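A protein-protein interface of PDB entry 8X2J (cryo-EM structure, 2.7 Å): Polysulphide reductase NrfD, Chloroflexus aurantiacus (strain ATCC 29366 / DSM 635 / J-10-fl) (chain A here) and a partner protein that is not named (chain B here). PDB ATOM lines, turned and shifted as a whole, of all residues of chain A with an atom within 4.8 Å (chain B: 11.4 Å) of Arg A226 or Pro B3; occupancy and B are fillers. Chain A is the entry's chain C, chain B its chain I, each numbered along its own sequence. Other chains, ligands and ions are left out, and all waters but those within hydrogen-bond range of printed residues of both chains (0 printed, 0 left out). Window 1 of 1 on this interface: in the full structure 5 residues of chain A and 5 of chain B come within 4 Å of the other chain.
Of the 9 printed residues of chain A, 4 touch a printed residue of chain B.
Printed residues of chain A that touch a printed residue of chain B: Arg A222, His A223, His A225 and Arg A226.
Hydrophobic or aromatic side chains of chain A that line the printed part of chain B: His A223 and His A225.
Of the 11 printed residues of chain B, 4 touch a printed residue of chain A.
Hydrophobic or aromatic side chains of chain B within 4 Å of the printed part of chain A: Met B1.
Among the printed residues, 6 pairs touch across the chains.
Among the printed residues, Asp or Glu carboxylates within 4 Å of a Lys or Arg side-chain nitrogen of the other chain: Arg A222 with Glu B4.
Among the printed residues, pairs that only touch across the chains: His A223 with Glu B4 (3.1 Å), His A225 with Met B1 (3.5 Å), Arg A226 with Met B1 (3.5 Å), Arg A226 with Gln B2 (3.7 Å) and Arg A226 with Pro B3 (3.9 Å).
O of Pro B3 lies within hydrogen-bond range of OG of Ser B6, 2.9 Å away.
The guanidinium group (NH1) of Arg A222 lies within salt-bridge range of the side-chain carboxylate (OE1) of Glu B4, 2.5 Å away.
Pro B3 touches one residue of chain A.
Of chain B, only Glu B4 (3.1 Å) comes within 4 Å of His A223.
Of the printed residues of chain B, Arg A222 touches Glu B4 (2.5 Å).
Of the printed residues of chain A, Gln B2 touches Arg A226.
Of the printed residues of chain A, Glu B4 touches Arg A222 and His A223.
Asp B8 touches none of the printed residues of chain A.
The nearest residue of chain B that does not touch Arg A226 is Glu B4 (4.5 Å).
The nearest printed residue of chain A that does not touch Pro B3 is Arg A222 (6.0 Å).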
ATOM      1  N   ARG A 222      24.254 -17.953 -15.208  1.00  0.00           N
ATOM      2  CA  ARG A 222      23.447 -18.441 -14.095  1.00  0.00           C
ATOM      3  C   ARG A 222      24.327 -19.048 -13.012  1.00  0.00           C
ATOM      4  O   ARG A 222      24.068 -18.869 -11.817  1.00  0.00           O
ATOM      5  CB  ARG A 222      22.427 -19.461 -14.597  1.00  0.00           C
ATOM      6  CG  ARG A 222      21.216 -18.847 -15.273  1.00  0.00           C
ATOM      7  CD  ARG A 222      20.113 -19.875 -15.481  1.00  0.00           C
ATOM      8  NE  ARG A 222      20.325 -20.679 -16.680  1.00  0.00           N
ATOM      9  CZ  ARG A 222      20.696 -21.951 -16.673  1.00  0.00           C
ATOM     10  NH1 ARG A 222      20.919 -22.600 -15.544  1.00  0.00           N
ATOM     11  NH2 ARG A 222      20.849 -22.587 -17.832  1.00  0.00           N
ATOM     12  N   HIS A 223      25.376 -19.765 -13.417  1.00  0.00           N
ATOM     13  CA  HIS A 223      26.316 -20.337 -12.461  1.00  0.00           C
ATOM     14  C   HIS A 223      27.210 -19.265 -11.856  1.00  0.00           C
ATOM     15  O   HIS A 223      27.669 -19.413 -10.718  1.00  0.00           O
ATOM     16  CB  HIS A 223      27.172 -21.409 -13.139  1.00  0.00           C
ATOM     17  CG  HIS A 223      26.419 -22.650 -13.512  1.00  0.00           C
ATOM     18  ND1 HIS A 223      25.239 -22.626 -14.222  1.00  0.00           N
ATOM     19  CD2 HIS A 223      26.697 -23.956 -13.294  1.00  0.00           C
ATOM     20  CE1 HIS A 223      24.817 -23.861 -14.418  1.00  0.00           C
ATOM     21  NE2 HIS A 223      25.680 -24.687 -13.858  1.00  0.00           N
ATOM     22  N   TRP A 224      27.468 -18.187 -12.601  1.00  0.00           N
ATOM     23  CA  TRP A 224      28.315 -17.116 -12.091  1.00  0.00           C
ATOM     24  C   TRP A 224      27.626 -16.322 -10.990  1.00  0.00           C
ATOM     25  O   TRP A 224      28.298 -15.824 -10.084  1.00  0.00           O
ATOM     26  CB  TRP A 224      28.740 -16.184 -13.228  1.00  0.00           C
ATOM     27  CG  TRP A 224      29.962 -16.630 -13.997  1.00  0.00           C
ATOM     28  CD1 TRP A 224      30.035 -16.874 -15.336  1.00  0.00           C
ATOM     29  CD2 TRP A 224      31.282 -16.864 -13.478  1.00  0.00           C
ATOM     30  NE1 TRP A 224      31.305 -17.255 -15.682  1.00  0.00           N
ATOM     31  CE2 TRP A 224      32.091 -17.255 -14.561  1.00  0.00           C
ATOM     32  CE3 TRP A 224      31.856 -16.784 -12.204  1.00  0.00           C
ATOM     33  CZ2 TRP A 224      33.439 -17.565 -14.411  1.00  0.00           C
ATOM     34  CZ3 TRP A 224      33.192 -17.094 -12.060  1.00  0.00           C
ATOM     35  CH2 TRP A 224      33.968 -17.478 -13.155  1.00  0.00           C
ATOM     36  N   HIS A 225      26.294 -16.211 -11.039  1.00  0.00           N
ATOM     37  CA  HIS A 225      25.551 -15.517  -9.990  1.00  0.00           C
ATOM     38  C   HIS A 225      25.637 -16.264  -8.664  1.00  0.00           C
ATOM     39  O   HIS A 225      25.948 -15.671  -7.620  1.00  0.00           O
ATOM     40  CB  HIS A 225      24.093 -15.353 -10.415  1.00  0.00           C
ATOM     41  CG  HIS A 225      23.351 -14.307  -9.644  1.00  0.00           C
ATOM     42  ND1 HIS A 225      21.988 -14.356  -9.447  1.00  0.00           N
ATOM     43  CD2 HIS A 225      23.781 -13.187  -9.019  1.00  0.00           C
ATOM     44  CE1 HIS A 225      21.610 -13.310  -8.736  1.00  0.00           C
ATOM     45  NE2 HIS A 225      22.679 -12.584  -8.462  1.00  0.00           N
ATOM     46  N   ARG A 226      25.378 -17.574  -8.696  1.00  0.00           N
ATOM     47  CA  ARG A 226      25.510 -18.405  -7.506  1.00  0.00           C
ATOM     48  C   ARG A 226      26.955 -18.488  -7.037  1.00  0.00           C
ATOM     49  O   ARG A 226      27.206 -18.531  -5.828  1.00  0.00           O
ATOM     50  CB  ARG A 226      24.966 -19.802  -7.783  1.00  0.00           C
ATOM     51  CG  ARG A 226      23.548 -20.013  -7.315  1.00  0.00           C
ATOM     52  CD  ARG A 226      22.986 -21.304  -7.851  1.00  0.00           C
ATOM     53  NE  ARG A 226      22.379 -21.139  -9.164  1.00  0.00           N
ATOM     54  CZ  ARG A 226      21.072 -21.137  -9.385  1.00  0.00           C
ATOM     55  NH1 ARG A 226      20.205 -21.275  -8.396  1.00  0.00           N
ATOM     56  NH2 ARG A 226      20.624 -20.996 -10.629  1.00  0.00           N
ATOM     57  N   TYR A 227      27.905 -18.490  -7.976  1.00  0.00           N
ATOM     58  CA  TYR A 227      29.321 -18.495  -7.628  1.00  0.00           C
ATOM     59  C   TYR A 227      29.728 -17.222  -6.903  1.00  0.00           C
ATOM     60  O   TYR A 227      30.452 -17.277  -5.902  1.00  0.00           O
ATOM     61  CB  TYR A 227      30.157 -18.669  -8.893  1.00  0.00           C
ATOM     62  CG  TYR A 227      31.619 -18.928  -8.641  1.00  0.00           C
ATOM     63  CD1 TYR A 227      32.078 -20.210  -8.380  1.00  0.00           C
ATOM     64  CD2 TYR A 227      32.544 -17.889  -8.673  1.00  0.00           C
ATOM     65  CE1 TYR A 227      33.412 -20.451  -8.151  1.00  0.00           C
ATOM     66  CE2 TYR A 227      33.878 -18.121  -8.442  1.00  0.00           C
ATOM     67  CZ  TYR A 227      34.305 -19.403  -8.183  1.00  0.00           C
ATOM     68  OH  TYR A 227      35.634 -19.636  -7.957  1.00  0.00           O
ATOM     69  N   GLU A 228      29.278 -16.065  -7.393  1.00  0.00           N
ATOM     70  CA  GLU A 228      29.624 -14.802  -6.753  1.00  0.00           C
ATOM     71  C   GLU A 228      28.947 -14.667  -5.395  1.00  0.00           C
ATOM     72  O   GLU A 228      29.554 -14.151  -4.451  1.00  0.00           O
ATOM     73  CB  GLU A 228      29.253 -13.630  -7.660  1.00  0.00           C
ATOM     74  CG  GLU A 228      30.192 -13.438  -8.843  1.00  0.00           C
ATOM     75  CD  GLU A 228      31.606 -13.083  -8.428  1.00  0.00           C
ATOM     76  OE1 GLU A 228      31.771 -12.300  -7.468  1.00  0.00           O
ATOM     77  OE2 GLU A 228      32.555 -13.586  -9.064  1.00  0.00           O
ATOM     78  N   MET A 229      27.701 -15.144  -5.273  1.00  0.00           N
ATOM     79  CA  MET A 229      27.030 -15.127  -3.975  1.00  0.00           C
ATOM     80  C   MET A 229      27.716 -16.049  -2.974  1.00  0.00           C
ATOM     81  O   MET A 229      27.875 -15.689  -1.801  1.00  0.00           O
ATOM     82  CB  MET A 229      25.561 -15.511  -4.130  1.00  0.00           C
ATOM     83  CG  MET A 229      24.705 -15.072  -2.956  1.00  0.00           C
ATOM     84  SD  MET A 229      24.698 -13.279  -2.770  1.00  0.00           S
ATOM     85  CE  MET A 229      25.011 -13.113  -1.017  1.00  0.00           C
ATOM     86  N   ALA A 230      28.141 -17.235  -3.421  1.00  0.00           N
ATOM     87  CA  ALA A 230      28.844 -18.161  -2.541  1.00  0.00           C
ATOM     88  C   ALA A 230      30.209 -17.626  -2.139  1.00  0.00           C
ATOM     89  O   ALA A 230      30.630 -17.807  -0.996  1.00  0.00           O
ATOM     90  CB  ALA A 230      28.995 -19.518  -3.215  1.00  0.00           C
ATOM     91  N   MET B   1      15.598 -16.670  -8.245  1.00  0.00           N
ATOM     92  CA  MET B   1      15.457 -17.459  -9.460  1.00  0.00           C
ATOM     93  C   MET B   1      15.323 -18.940  -9.136  1.00  0.00           C
ATOM     94  O   MET B   1      15.648 -19.377  -8.032  1.00  0.00           O
ATOM     95  CB  MET B   1      16.648 -17.228 -10.393  1.00  0.00           C
ATOM     96  CG  MET B   1      17.980 -17.692  -9.832  1.00  0.00           C
ATOM     97  SD  MET B   1      19.371 -17.268 -10.899  1.00  0.00           S
ATOM     98  CE  MET B   1      20.749 -17.559  -9.795  1.00  0.00           C
ATOM     99  N   GLN B   2      14.834 -19.705 -10.107  1.00  0.00           N
ATOM    100  CA  GLN B   2      14.656 -21.134  -9.926  1.00  0.00           C
ATOM    101  C   GLN B   2      16.011 -21.843  -9.928  1.00  0.00           C
ATOM    102  O   GLN B   2      16.978 -21.342 -10.507  1.00  0.00           O
ATOM    103  CB  GLN B   2      13.764 -21.697 -11.032  1.00  0.00           C
ATOM    104  CG  GLN B   2      12.319 -21.234 -10.955  1.00  0.00           C
ATOM    105  CD  GLN B   2      11.516 -21.998  -9.920  1.00  0.00           C
ATOM    106  OE1 GLN B   2      11.935 -23.053  -9.447  1.00  0.00           O
ATOM    107  NE2 GLN B   2      10.353 -21.465  -9.565  1.00  0.00           N
ATOM    108  N   PRO B   3      16.114 -23.000  -9.273  1.00  0.00           N
ATOM    109  CA  PRO B   3      17.354 -23.783  -9.345  1.00  0.00           C
ATOM    110  C   PRO B   3      17.550 -24.412 -10.717  1.00  0.00           C
ATOM    111  O   PRO B   3      16.698 -24.343 -11.606  1.00  0.00           O
ATOM    112  CB  PRO B   3      17.168 -24.852  -8.266  1.00  0.00           C
ATOM    113  CG  PRO B   3      15.704 -24.933  -8.055  1.00  0.00           C
ATOM    114  CD  PRO B   3      15.199 -23.541  -8.253  1.00  0.00           C
ATOM    115  N   GLU B   4      18.719 -25.038 -10.876  1.00  0.00           N
ATOM    116  CA  GLU B   4      19.087 -25.637 -12.155  1.00  0.00           C
ATOM    117  C   GLU B   4      18.239 -26.863 -12.466  1.00  0.00           C
ATOM    118  O   GLU B   4      17.803 -27.051 -13.608  1.00  0.00           O
ATOM    119  CB  GLU B   4      20.569 -26.003 -12.145  1.00  0.00           C
ATOM    120  CG  GLU B   4      21.077 -26.632 -13.429  1.00  0.00           C
ATOM    121  CD  GLU B   4      21.470 -25.599 -14.462  1.00  0.00           C
ATOM    122  OE1 GLU B   4      21.749 -24.447 -14.071  1.00  0.00           O
ATOM    123  OE2 GLU B   4      21.503 -25.941 -15.663  1.00  0.00           O
ATOM    124  N   TRP B   5      17.984 -27.699 -11.464  1.00  0.00           N
ATOM    125  CA  TRP B   5      17.244 -28.936 -11.651  1.00  0.00           C
ATOM    126  C   TRP B   5      15.750 -28.780 -11.392  1.00  0.00           C
ATOM    127  O   TRP B   5      15.069 -29.782 -11.153  1.00  0.00           O
ATOM    128  CB  TRP B   5      17.823 -30.032 -10.754  1.00  0.00           C
ATOM    129  CG  TRP B   5      18.406 -29.522  -9.471  1.00  0.00           C
ATOM    130  CD1 TRP B   5      19.726 -29.352  -9.186  1.00  0.00           C
ATOM    131  CD2 TRP B   5      17.688 -29.121  -8.299  1.00  0.00           C
ATOM    132  NE1 TRP B   5      19.878 -28.869  -7.910  1.00  0.00           N
ATOM    133  CE2 TRP B   5      18.640 -28.717  -7.344  1.00  0.00           C
ATOM    134  CE3 TRP B   5      16.331 -29.061  -7.965  1.00  0.00           C
ATOM    135  CZ2 TRP B   5      18.282 -28.263  -6.078  1.00  0.00           C
ATOM    136  CZ3 TRP B   5      15.978 -28.610  -6.709  1.00  0.00           C
ATOM    137  CH2 TRP B   5      16.949 -28.216  -5.780  1.00  0.00           C
ATOM    138  N   SER B   6      15.227 -27.556 -11.434  1.00  0.00           N
ATOM    139  CA  SER B   6      13.804 -27.344 -11.203  1.00  0.00           C
ATOM    140  C   SER B   6      12.992 -27.885 -12.374  1.00  0.00           C
ATOM    141  O   SER B   6      13.286 -27.595 -13.537  1.00  0.00           O
ATOM    142  CB  SER B   6      13.515 -25.859 -10.994  1.00  0.00           C
ATOM    143  OG  SER B   6      13.943 -25.091 -12.106  1.00  0.00           O
ATOM    144  N   GLY B   7      11.969 -28.676 -12.061  1.00  0.00           N
ATOM    145  CA  GLY B   7      11.167 -29.326 -13.073  1.00  0.00           C
ATOM    146  C   GLY B   7      11.628 -30.708 -13.475  1.00  0.00           C
ATOM    147  O   GLY B   7      11.057 -31.286 -14.407  1.00  0.00           O
ATOM    148  N   ASP B   8      12.642 -31.260 -12.802  1.00  0.00           N
ATOM    149  CA  ASP B   8      13.162 -32.591 -13.096  1.00  0.00           C
ATOM    150  C   ASP B   8      12.455 -33.625 -12.238  1.00  0.00           C
ATOM    151  O   ASP B   8      12.367 -33.445 -11.015  1.00  0.00           O
ATOM    152  CB  ASP B   8      14.665 -32.648 -12.837  1.00  0.00           C
ATOM    153  CG  ASP B   8      15.396 -33.536 -13.825  1.00  0.00           C
ATOM    154  OD1 ASP B   8      14.823 -33.846 -14.889  1.00  0.00           O
ATOM    155  OD2 ASP B   8      16.547 -33.925 -13.537  1.00  0.00           O
ATOM    156  N   VAL B  11      14.317 -35.237  -8.996  1.00  0.00           N
ATOM    157  CA  VAL B  11      14.795 -34.397  -7.899  1.00  0.00           C
ATOM    158  C   VAL B  11      14.249 -34.883  -6.561  1.00  0.00           C
ATOM    159  O   VAL B  11      14.994 -35.023  -5.584  1.00  0.00           O
ATOM    160  CB  VAL B  11      14.429 -32.926  -8.169  1.00  0.00           C
ATOM    161  CG1 VAL B  11      14.457 -32.092  -6.893  1.00  0.00           C
ATOM    162  CG2 VAL B  11      15.381 -32.360  -9.179  1.00  0.00           C
ATOM    163  N   LYS B  12      12.957 -35.168  -6.496  1.00  0.00           N
ATOM    164  CA  LYS B  12      12.415 -35.656  -5.233  1.00  0.00           C
ATOM    165  C   LYS B  12      12.797 -37.116  -4.955  1.00  0.00           C
ATOM    166  O   LYS B  12      13.026 -37.436  -3.781  1.00  0.00           O
ATOM    167  CB  LYS B  12      10.895 -35.436  -5.174  1.00  0.00           C
ATOM    168  CG  LYS B  12      10.496 -33.985  -4.963  1.00  0.00           C
ATOM    169  CD  LYS B  12       9.061 -33.856  -4.480  1.00  0.00           C
ATOM    170  CE  LYS B  12       8.692 -32.398  -4.247  1.00  0.00           C
ATOM    171  NZ  LYS B  12       7.340 -32.252  -3.642  1.00  0.00           N
ATOM    172  N   PHE B  15      16.311 -36.620  -3.561  1.00  0.00           N
ATOM    173  CA  PHE B  15      16.263 -36.028  -2.227  1.00  0.00           C
ATOM    174  C   PHE B  15      15.823 -37.042  -1.180  1.00  0.00           C
ATOM    175  O   PHE B  15      16.386 -37.083  -0.080  1.00  0.00           O
ATOM    176  CB  PHE B  15      15.337 -34.809  -2.211  1.00  0.00           C
ATOM    177  CG  PHE B  15      15.961 -33.555  -2.765  1.00  0.00           C
ATOM    178  CD1 PHE B  15      17.321 -33.490  -3.031  1.00  0.00           C
ATOM    179  CD2 PHE B  15      15.184 -32.431  -3.003  1.00  0.00           C
ATOM    180  CE1 PHE B  15      17.892 -32.334  -3.532  1.00  0.00           C
ATOM    181  CE2 PHE B  15      15.747 -31.271  -3.505  1.00  0.00           C
ATOM    182  CZ  PHE B  15      17.103 -31.224  -3.768  1.00  0.00           C
